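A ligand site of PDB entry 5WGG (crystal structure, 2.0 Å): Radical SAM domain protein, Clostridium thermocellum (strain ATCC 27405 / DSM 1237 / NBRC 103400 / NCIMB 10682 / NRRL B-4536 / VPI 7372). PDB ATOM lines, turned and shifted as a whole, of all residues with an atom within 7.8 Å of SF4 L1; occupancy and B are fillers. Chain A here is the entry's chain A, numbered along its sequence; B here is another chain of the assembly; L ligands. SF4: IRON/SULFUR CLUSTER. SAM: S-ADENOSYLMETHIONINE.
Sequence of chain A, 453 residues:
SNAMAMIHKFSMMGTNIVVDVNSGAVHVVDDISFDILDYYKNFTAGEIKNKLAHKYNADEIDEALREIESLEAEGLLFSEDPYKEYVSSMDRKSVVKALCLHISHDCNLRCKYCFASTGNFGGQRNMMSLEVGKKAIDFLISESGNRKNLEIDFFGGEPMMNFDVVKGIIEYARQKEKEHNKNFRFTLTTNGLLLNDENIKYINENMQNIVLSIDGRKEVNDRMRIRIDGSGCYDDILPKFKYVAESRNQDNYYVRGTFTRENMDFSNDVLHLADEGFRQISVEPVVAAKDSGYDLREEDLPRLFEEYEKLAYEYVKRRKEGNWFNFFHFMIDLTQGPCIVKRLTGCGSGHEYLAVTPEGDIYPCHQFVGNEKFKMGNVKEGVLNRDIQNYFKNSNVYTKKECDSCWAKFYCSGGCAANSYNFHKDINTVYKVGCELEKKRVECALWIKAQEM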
ATOM      1  N   ARG A 256     -19.630  23.679  -1.696  1.00  0.00           N
ATOM      2  CA  ARG A 256     -18.837  22.667  -2.387  1.00  0.00           C
ATOM      3  C   ARG A 256     -18.976  22.853  -3.896  1.00  0.00           C
ATOM      4  O   ARG A 256     -20.064  22.671  -4.463  1.00  0.00           O
ATOM      5  CB  ARG A 256     -19.284  21.271  -1.951  1.00  0.00           C
ATOM      6  CG  ARG A 256     -18.860  20.100  -2.865  1.00  0.00           C
ATOM      7  CD  ARG A 256     -17.390  19.760  -2.814  1.00  0.00           C
ATOM      8  NE  ARG A 256     -17.224  18.345  -3.160  1.00  0.00           N
ATOM      9  CZ  ARG A 256     -17.287  17.857  -4.397  1.00  0.00           C
ATOM     10  NH1 ARG A 256     -17.477  18.672  -5.429  1.00  0.00           N
ATOM     11  NH2 ARG A 256     -17.162  16.557  -4.614  1.00  0.00           N
ATOM     12  N   GLU A 284     -13.237  21.362  -5.922  1.00  0.00           N
ATOM     13  CA  GLU A 284     -12.479  20.144  -6.174  1.00  0.00           C
ATOM     14  C   GLU A 284     -12.542  19.750  -7.645  1.00  0.00           C
ATOM     15  O   GLU A 284     -13.541  20.025  -8.327  1.00  0.00           O
ATOM     16  CB  GLU A 284     -13.025  18.989  -5.305  1.00  0.00           C
ATOM     17  CG  GLU A 284     -13.177  19.409  -3.837  1.00  0.00           C
ATOM     18  CD  GLU A 284     -13.800  18.339  -2.945  1.00  0.00           C
ATOM     19  OE1 GLU A 284     -14.334  18.719  -1.865  1.00  0.00           O
ATOM     20  OE2 GLU A 284     -13.739  17.127  -3.306  1.00  0.00           O
ATOM     21  N   VAL A 287     -14.541  14.206 -10.758  1.00  0.00           N
ATOM     22  CA  VAL A 287     -14.199  12.795 -10.611  1.00  0.00           C
ATOM     23  C   VAL A 287     -14.809  11.995 -11.765  1.00  0.00           C
ATOM     24  O   VAL A 287     -15.954  12.258 -12.181  1.00  0.00           O
ATOM     25  CB  VAL A 287     -14.703  12.257  -9.261  1.00  0.00           C
ATOM     26  CG1 VAL A 287     -14.577  10.735  -9.192  1.00  0.00           C
ATOM     27  CG2 VAL A 287     -13.970  12.970  -8.069  1.00  0.00           C
ATOM     28  N   ALA A 288     -14.060  11.011 -12.270  1.00  0.00           N
ATOM     29  CA  ALA A 288     -14.565   9.984 -13.201  1.00  0.00           C
ATOM     30  C   ALA A 288     -15.145  10.597 -14.480  1.00  0.00           C
ATOM     31  O   ALA A 288     -16.220  10.221 -14.947  1.00  0.00           O
ATOM     32  CB  ALA A 288     -15.580   9.074 -12.505  1.00  0.00           C
ATOM     33  N   GLY A 346      -7.168   5.761   3.458  1.00  0.00           N
ATOM     34  CA  GLY A 346      -7.669   6.570   2.348  1.00  0.00           C
ATOM     35  C   GLY A 346      -9.066   7.107   2.623  1.00  0.00           C
ATOM     36  O   GLY A 346      -9.466   7.242   3.783  1.00  0.00           O
ATOM     37  N   CYS A 347      -9.825   7.384   1.553  1.00  0.00           N
ATOM     38  CA  CYS A 347     -11.233   7.776   1.707  1.00  0.00           C
ATOM     39  C   CYS A 347     -12.073   6.667   2.333  1.00  0.00           C
ATOM     40  O   CYS A 347     -13.154   6.932   2.867  1.00  0.00           O
ATOM     41  CB  CYS A 347     -11.865   8.157   0.348  1.00  0.00           C
ATOM     42  SG  CYS A 347     -11.979   6.649  -0.708  1.00  0.00           S
ATOM     43  N   GLY A 348     -11.625   5.420   2.249  1.00  0.00           N
ATOM     44  CA  GLY A 348     -12.301   4.304   2.868  1.00  0.00           C
ATOM     45  C   GLY A 348     -13.359   3.610   2.018  1.00  0.00           C
ATOM     46  O   GLY A 348     -14.035   2.701   2.525  1.00  0.00           O
ATOM     47  N   SER A 349     -13.550   4.024   0.775  1.00  0.00           N
ATOM     48  CA  SER A 349     -14.611   3.427  -0.047  1.00  0.00           C
ATOM     49  C   SER A 349     -14.385   1.929  -0.226  1.00  0.00           C
ATOM     50  O   SER A 349     -13.243   1.465  -0.350  1.00  0.00           O
ATOM     51  CB  SER A 349     -14.716   4.130  -1.400  1.00  0.00           C
ATOM     52  OG  SER A 349     -13.463   4.156  -2.043  1.00  0.00           O
ATOM     53  N   GLY A 350     -15.461   1.148  -0.190  1.00  0.00           N
ATOM     54  CA  GLY A 350     -15.368  -0.293  -0.331  1.00  0.00           C
ATOM     55  C   GLY A 350     -15.081  -1.069   0.942  1.00  0.00           C
ATOM     56  O   GLY A 350     -15.309  -2.278   0.971  1.00  0.00           O
ATOM     57  N   TYR A 353     -16.196   2.826   4.295  1.00  0.00           N
ATOM     58  CA  TYR A 353     -17.185   3.798   3.884  1.00  0.00           C
ATOM     59  C   TYR A 353     -17.923   3.162   2.715  1.00  0.00           C
ATOM     60  O   TYR A 353     -17.276   2.690   1.777  1.00  0.00           O
ATOM     61  CB  TYR A 353     -16.485   5.092   3.489  1.00  0.00           C
ATOM     62  CG  TYR A 353     -17.358   6.152   2.891  1.00  0.00           C
ATOM     63  CD1 TYR A 353     -18.226   6.891   3.665  1.00  0.00           C
ATOM     64  CD2 TYR A 353     -17.283   6.441   1.532  1.00  0.00           C
ATOM     65  CE1 TYR A 353     -19.018   7.904   3.092  1.00  0.00           C
ATOM     66  CE2 TYR A 353     -18.062   7.444   0.953  1.00  0.00           C
ATOM     67  CZ  TYR A 353     -18.921   8.167   1.744  1.00  0.00           C
ATOM     68  OH  TYR A 353     -19.676   9.139   1.153  1.00  0.00           O
ATOM     69  N   PRO A 364     -19.281   0.367  -3.041  1.00  0.00           N
ATOM     70  CA  PRO A 364     -18.134   1.012  -2.361  1.00  0.00           C
ATOM     71  C   PRO A 364     -18.319   2.486  -2.106  1.00  0.00           C
ATOM     72  O   PRO A 364     -17.959   2.990  -1.025  1.00  0.00           O
ATOM     73  CB  PRO A 364     -16.980   0.782  -3.335  1.00  0.00           C
ATOM     74  CG  PRO A 364     -17.365  -0.510  -4.026  1.00  0.00           C
ATOM     75  CD  PRO A 364     -18.855  -0.401  -4.221  1.00  0.00           C
ATOM     76  N   CYS A 365     -18.859   3.213  -3.084  1.00  0.00           N
ATOM     77  CA  CYS A 365     -19.168   4.624  -2.894  1.00  0.00           C
ATOM     78  C   CYS A 365     -20.148   5.018  -3.992  1.00  0.00           C
ATOM     79  O   CYS A 365     -20.479   4.232  -4.890  1.00  0.00           O
ATOM     80  CB  CYS A 365     -17.913   5.522  -2.941  1.00  0.00           C
ATOM     81  SG  CYS A 365     -17.335   5.806  -4.621  1.00  0.00           S
ATOM     82  N   HIS A 366     -20.583   6.278  -3.922  1.00  0.00           N
ATOM     83  CA  HIS A 366     -21.576   6.739  -4.879  1.00  0.00           C
ATOM     84  C   HIS A 366     -21.073   6.646  -6.319  1.00  0.00           C
ATOM     85  O   HIS A 366     -21.894   6.511  -7.220  1.00  0.00           O
ATOM     86  CB  HIS A 366     -21.996   8.170  -4.554  1.00  0.00           C
ATOM     87  CG  HIS A 366     -21.006   9.202  -4.995  1.00  0.00           C
ATOM     88  ND1 HIS A 366     -21.221  10.015  -6.084  1.00  0.00           N
ATOM     89  CD2 HIS A 366     -19.794   9.528  -4.512  1.00  0.00           C
ATOM     90  CE1 HIS A 366     -20.188  10.813  -6.249  1.00  0.00           C
ATOM     91  NE2 HIS A 366     -19.293  10.543  -5.303  1.00  0.00           N
ATOM     92  N   GLN A 367     -19.767   6.683  -6.558  1.00  0.00           N
ATOM     93  CA  GLN A 367     -19.333   6.627  -7.954  1.00  0.00           C
ATOM     94  C   GLN A 367     -19.392   5.230  -8.548  1.00  0.00           C
ATOM     95  O   GLN A 367     -19.300   5.086  -9.772  1.00  0.00           O
ATOM     96  CB  GLN A 367     -17.913   7.193  -8.076  1.00  0.00           C
ATOM     97  CG  GLN A 367     -17.795   8.707  -7.830  1.00  0.00           C
ATOM     98  CD  GLN A 367     -18.273   9.525  -9.023  1.00  0.00           C
ATOM     99  OE1 GLN A 367     -18.344   9.028 -10.142  1.00  0.00           O
ATOM    100  NE2 GLN A 367     -18.601  10.784  -8.799  1.00  0.00           N
ATOM    101  N   PHE A 368     -19.588   4.196  -7.738  1.00  0.00           N
ATOM    102  CA  PHE A 368     -19.685   2.831  -8.243  1.00  0.00           C
ATOM    103  C   PHE A 368     -21.123   2.318  -8.311  1.00  0.00           C
ATOM    104  O   PHE A 368     -21.336   1.223  -8.840  1.00  0.00           O
ATOM    105  CB  PHE A 368     -18.883   1.868  -7.352  1.00  0.00           C
ATOM    106  CG  PHE A 368     -17.404   2.033  -7.442  1.00  0.00           C
ATOM    107  CD1 PHE A 368     -16.683   1.376  -8.422  1.00  0.00           C
ATOM    108  CD2 PHE A 368     -16.730   2.860  -6.536  1.00  0.00           C
ATOM    109  CE1 PHE A 368     -15.304   1.528  -8.499  1.00  0.00           C
ATOM    110  CE2 PHE A 368     -15.342   3.010  -6.608  1.00  0.00           C
ATOM    111  CZ  PHE A 368     -14.635   2.331  -7.577  1.00  0.00           C
ATOM    112  N   PHE A 392     -10.850  -3.755  -1.728  1.00  0.00           N
ATOM    113  CA  PHE A 392     -10.687  -2.306  -1.611  1.00  0.00           C
ATOM    114  C   PHE A 392      -9.798  -1.944  -0.418  1.00  0.00           C
ATOM    115  O   PHE A 392      -8.919  -1.089  -0.534  1.00  0.00           O
ATOM    116  CB  PHE A 392     -12.053  -1.629  -1.487  1.00  0.00           C
ATOM    117  CG  PHE A 392     -12.727  -1.348  -2.808  1.00  0.00           C
ATOM    118  CD1 PHE A 392     -13.292  -2.388  -3.546  1.00  0.00           C
ATOM    119  CD2 PHE A 392     -12.827  -0.044  -3.285  1.00  0.00           C
ATOM    120  CE1 PHE A 392     -13.929  -2.150  -4.759  1.00  0.00           C
ATOM    121  CE2 PHE A 392     -13.458   0.219  -4.514  1.00  0.00           C
ATOM    122  CZ  PHE A 392     -13.989  -0.845  -5.257  1.00  0.00           C
ATOM    123  N   SER A 413      -4.505  12.154   0.121  1.00  0.00           N
ATOM    124  CA  SER A 413      -5.713  11.542   0.642  1.00  0.00           C
ATOM    125  C   SER A 413      -5.803  10.061   0.259  1.00  0.00           C
ATOM    126  O   SER A 413      -6.799   9.419   0.604  1.00  0.00           O
ATOM    127  CB  SER A 413      -6.950  12.288   0.132  1.00  0.00           C
ATOM    128  OG  SER A 413      -7.007  12.262  -1.279  1.00  0.00           O
ATOM    129  N   GLY A 414      -4.816   9.532  -0.453  1.00  0.00           N
ATOM    130  CA  GLY A 414      -4.753   8.121  -0.774  1.00  0.00           C
ATOM    131  C   GLY A 414      -5.187   7.744  -2.186  1.00  0.00           C
ATOM    132  O   GLY A 414      -5.113   6.567  -2.532  1.00  0.00           O
ATOM    133  N   GLY A 415      -5.577   8.708  -3.025  1.00  0.00           N
ATOM    134  CA  GLY A 415      -6.075   8.384  -4.338  1.00  0.00           C
ATOM    135  C   GLY A 415      -7.561   8.105  -4.287  1.00  0.00           C
ATOM    136  O   GLY A 415      -8.211   8.120  -3.232  1.00  0.00           O
ATOM    137  N   CYS A 416      -8.113   7.886  -5.457  1.00  0.00           N
ATOM    138  CA  CYS A 416      -9.558   7.790  -5.606  1.00  0.00           C
ATOM    139  C   CYS A 416      -9.800   6.584  -6.489  1.00  0.00           C
ATOM    140  O   CYS A 416      -9.491   6.596  -7.689  1.00  0.00           O
ATOM    141  CB  CYS A 416     -10.131   9.094  -6.192  1.00  0.00           C
ATOM    142  SG  CYS A 416     -11.868   9.020  -6.764  1.00  0.00           S
ATOM    143  N   ALA A 417     -10.297   5.516  -5.855  1.00  0.00           N
ATOM    144  CA  ALA A 417     -10.620   4.278  -6.540  1.00  0.00           C
ATOM    145  C   ALA A 417     -11.543   4.504  -7.739  1.00  0.00           C
ATOM    146  O   ALA A 417     -11.401   3.857  -8.779  1.00  0.00           O
ATOM    147  CB  ALA A 417     -11.244   3.312  -5.530  1.00  0.00           C
ATOM    148  N   ALA A 418     -12.485   5.430  -7.599  1.00  0.00           N
ATOM    149  CA  ALA A 418     -13.406   5.732  -8.695  1.00  0.00           C
ATOM    150  C   ALA A 418     -12.640   6.256  -9.906  1.00  0.00           C
ATOM    151  O   ALA A 418     -12.826   5.760 -11.021  1.00  0.00           O
ATOM    152  CB  ALA A 418     -14.439   6.746  -8.218  1.00  0.00           C
ATOM    153  N   ASN A 419     -11.739   7.234  -9.709  1.00  0.00           N
ATOM    154  CA  ASN A 419     -10.908   7.702 -10.819  1.00  0.00           C
ATOM    155  C   ASN A 419     -10.104   6.556 -11.402  1.00  0.00           C
ATOM    156  O   ASN A 419     -10.081   6.346 -12.625  1.00  0.00           O
ATOM    157  CB  ASN A 419      -9.964   8.826 -10.364  1.00  0.00           C
ATOM    158  CG  ASN A 419     -10.652  10.211 -10.343  1.00  0.00           C
ATOM    159  OD1 ASN A 419     -11.643  10.428 -11.043  1.00  0.00           O
ATOM    160  ND2 ASN A 419     -10.089  11.163  -9.585  1.00  0.00           N
ATOM    161  N   SER A 420      -9.452   5.783 -10.536  1.00  0.00           N
ATOM    162  CA  SER A 420      -8.638   4.665 -10.993  1.00  0.00           C
ATOM    163  C   SER A 420      -9.458   3.697 -11.856  1.00  0.00           C
ATOM    164  O   SER A 420      -9.048   3.349 -12.958  1.00  0.00           O
ATOM    165  CB  SER A 420      -8.025   3.971  -9.779  1.00  0.00           C
ATOM    166  OG  SER A 420      -6.979   4.781  -9.244  1.00  0.00           O
ATOM    167  N   ILE A 427      -8.825  -0.469  -9.799  1.00  0.00           N
ATOM    168  CA  ILE A 427      -8.707   0.466  -8.705  1.00  0.00           C
ATOM    169  C   ILE A 427      -7.258   0.624  -8.242  1.00  0.00           C
ATOM    170  O   ILE A 427      -6.939   1.628  -7.615  1.00  0.00           O
ATOM    171  CB  ILE A 427      -9.627   0.082  -7.519  1.00  0.00           C
ATOM    172  CG1 ILE A 427      -9.170  -1.229  -6.857  1.00  0.00           C
ATOM    173  CG2 ILE A 427     -11.097   0.007  -7.971  1.00  0.00           C
ATOM    174  CD1 ILE A 427      -9.779  -1.448  -5.488  1.00  0.00           C
ATOM    175  N   GLY B  20     -14.315  17.007   0.622  1.00  0.00           N
ATOM    176  CA  GLY B  20     -14.091  15.803  -0.157  1.00  0.00           C
ATOM    177  C   GLY B  20     -15.199  14.755  -0.118  1.00  0.00           C
ATOM    178  O   GLY B  20     -16.338  15.030  -0.502  1.00  0.00           O
ATOM    179  N   CYS B  21     -14.853  13.545   0.331  1.00  0.00           N
ATOM    180  CA  CYS B  21     -15.819  12.459   0.492  1.00  0.00           C
ATOM    181  C   CYS B  21     -15.712  11.854   1.903  1.00  0.00           C
ATOM    182  O   CYS B  21     -15.761  10.635   2.086  1.00  0.00           O
ATOM    183  CB  CYS B  21     -15.607  11.367  -0.588  1.00  0.00           C
ATOM    184  SG  CYS B  21     -15.969  11.869  -2.328  1.00  0.00           S
HETATM  185 FE1  SF4 L   1     -14.803   9.728  -3.125  1.00  0.00          FE
HETATM  186 FE2  SF4 L   1     -13.156   8.463  -4.964  1.00  0.00          FE
HETATM  187 FE3  SF4 L   1     -15.462   7.237  -4.043  1.00  0.00          FE
HETATM  188 FE4  SF4 L   1     -13.289   7.651  -2.427  1.00  0.00          FE
HETATM  189  S1  SF4 L   1     -13.509   6.374  -4.271  1.00  0.00           S
HETATM  190  S2  SF4 L   1     -15.361   8.014  -1.950  1.00  0.00           S
HETATM  191  S3  SF4 L   1     -12.623   9.625  -3.137  1.00  0.00           S
HETATM  192  S4  SF4 L   1     -15.238   9.089  -5.162  1.00  0.00           S
HETATM  193  N   SAM L   2     -28.088  16.536  -4.443  1.00  0.00           N
HETATM  194  CA  SAM L   2     -27.060  16.821  -3.450  1.00  0.00           C
HETATM  195  C   SAM L   2     -26.125  17.973  -3.886  1.00  0.00           C
HETATM  196  O   SAM L   2     -25.970  18.319  -5.063  1.00  0.00           O
HETATM  197  OXT SAM L   2     -25.496  18.602  -3.036  1.00  0.00           O
HETATM  198  CB  SAM L   2     -26.276  15.556  -3.103  1.00  0.00           C
HETATM  199  CG  SAM L   2     -25.836  14.718  -4.298  1.00  0.00           C
HETATM  200  SD  SAM L   2     -24.570  15.472  -5.339  1.00  0.00           S
HETATM  201  CE  SAM L   2     -23.709  14.065  -6.101  1.00  0.00           C
HETATM  202  C5' SAM L   2     -23.321  15.904  -4.058  1.00  0.00           C
HETATM  203  C4' SAM L   2     -22.046  16.652  -4.492  1.00  0.00           C
HETATM  204  O4' SAM L   2     -21.227  15.871  -5.360  1.00  0.00           O
HETATM  205  C3' SAM L   2     -22.380  17.934  -5.257  1.00  0.00           C
HETATM  206  O3' SAM L   2     -21.631  19.038  -4.761  1.00  0.00           O
HETATM  207  C2' SAM L   2     -21.913  17.637  -6.660  1.00  0.00           C
HETATM  208  O2' SAM L   2     -21.457  18.801  -7.282  1.00  0.00           O
HETATM  209  C1' SAM L   2     -20.760  16.669  -6.415  1.00  0.00           C
HETATM  210  N9  SAM L   2     -20.463  15.894  -7.628  1.00  0.00           N
HETATM  211  C8  SAM L   2     -21.389  15.306  -8.462  1.00  0.00           C
HETATM  212  N7  SAM L   2     -20.714  14.683  -9.470  1.00  0.00           N
HETATM  213  C5  SAM L   2     -19.384  14.849  -9.305  1.00  0.00           C
HETATM  214  C6  SAM L   2     -18.255  14.432 -10.031  1.00  0.00           C
HETATM  215  N6  SAM L   2     -18.338  13.737 -11.144  1.00  0.00           N
HETATM  216  N1  SAM L   2     -16.995  14.779  -9.609  1.00  0.00           N
HETATM  217  C2  SAM L   2     -16.865  15.533  -8.464  1.00  0.00           C
HETATM  218  N3  SAM L   2     -17.976  15.941  -7.751  1.00  0.00           N
HETATM  219  C4  SAM L   2     -19.215  15.628  -8.152  1.00  0.00           C
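S1 of SF4 L1 lies close to OG of Ser 349, at 3.1 Å.
O of Val 287 is in hydrogen-bond range of N6 of SAM L2 (3.0 Å).
The side-chain sulfur (SG) of Cys 365 is bound to an iron atom (FE3) of SF4 L1, at 2.4 Å.
The side-chain sulfur (SG) of Cys 416 is bound to an iron atom (FE2) of SF4 L1 (2.3 Å).
The side-chain sulfur of Cys 347 is bound to an iron atom (FE4) of SF4 L1, 2.4 Å away.
The side-chain sulfur (SG) of Cys 21 of chain B binds an iron atom (FE1) of SF4 L1 (2.6 Å).
S1 of SF4 L1 sits close to N of Ala 418 (3.6 Å).
NH2 of Arg 256 lies within hydrogen-bond range of N3 of SAM L2, 3.3 Å away.
The backbone NH of Val 287 sits at hydrogen-bond distance from a nitrogen (N1) of SAM L2.
The backbone NH (N) of Ala 417 sits close to a sulfur (S1) of SF4 L1 (3.7 Å).
The backbone NH of Gln 367 sits close to the side-chain sulfur of Cys 365 (3.2 Å).
N of Asn 419 sits close to SG of Cys 416 (3.4 Å).
The side-chain sulfur (SG) of Cys 416 sits close to the backbone NH (N) of Ala 418 (3.7 Å).
The side-chain sulfur (SG) of Cys 347 sits close to the side-chain hydroxyl (OG) of Ser 349, 3.2 Å away.
OG of Ser 420 lies within hydrogen-bond range of O of Cys 416 (3.5 Å).
Residues that only touch SF4 L1: Gln 367 (3.7 Å).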
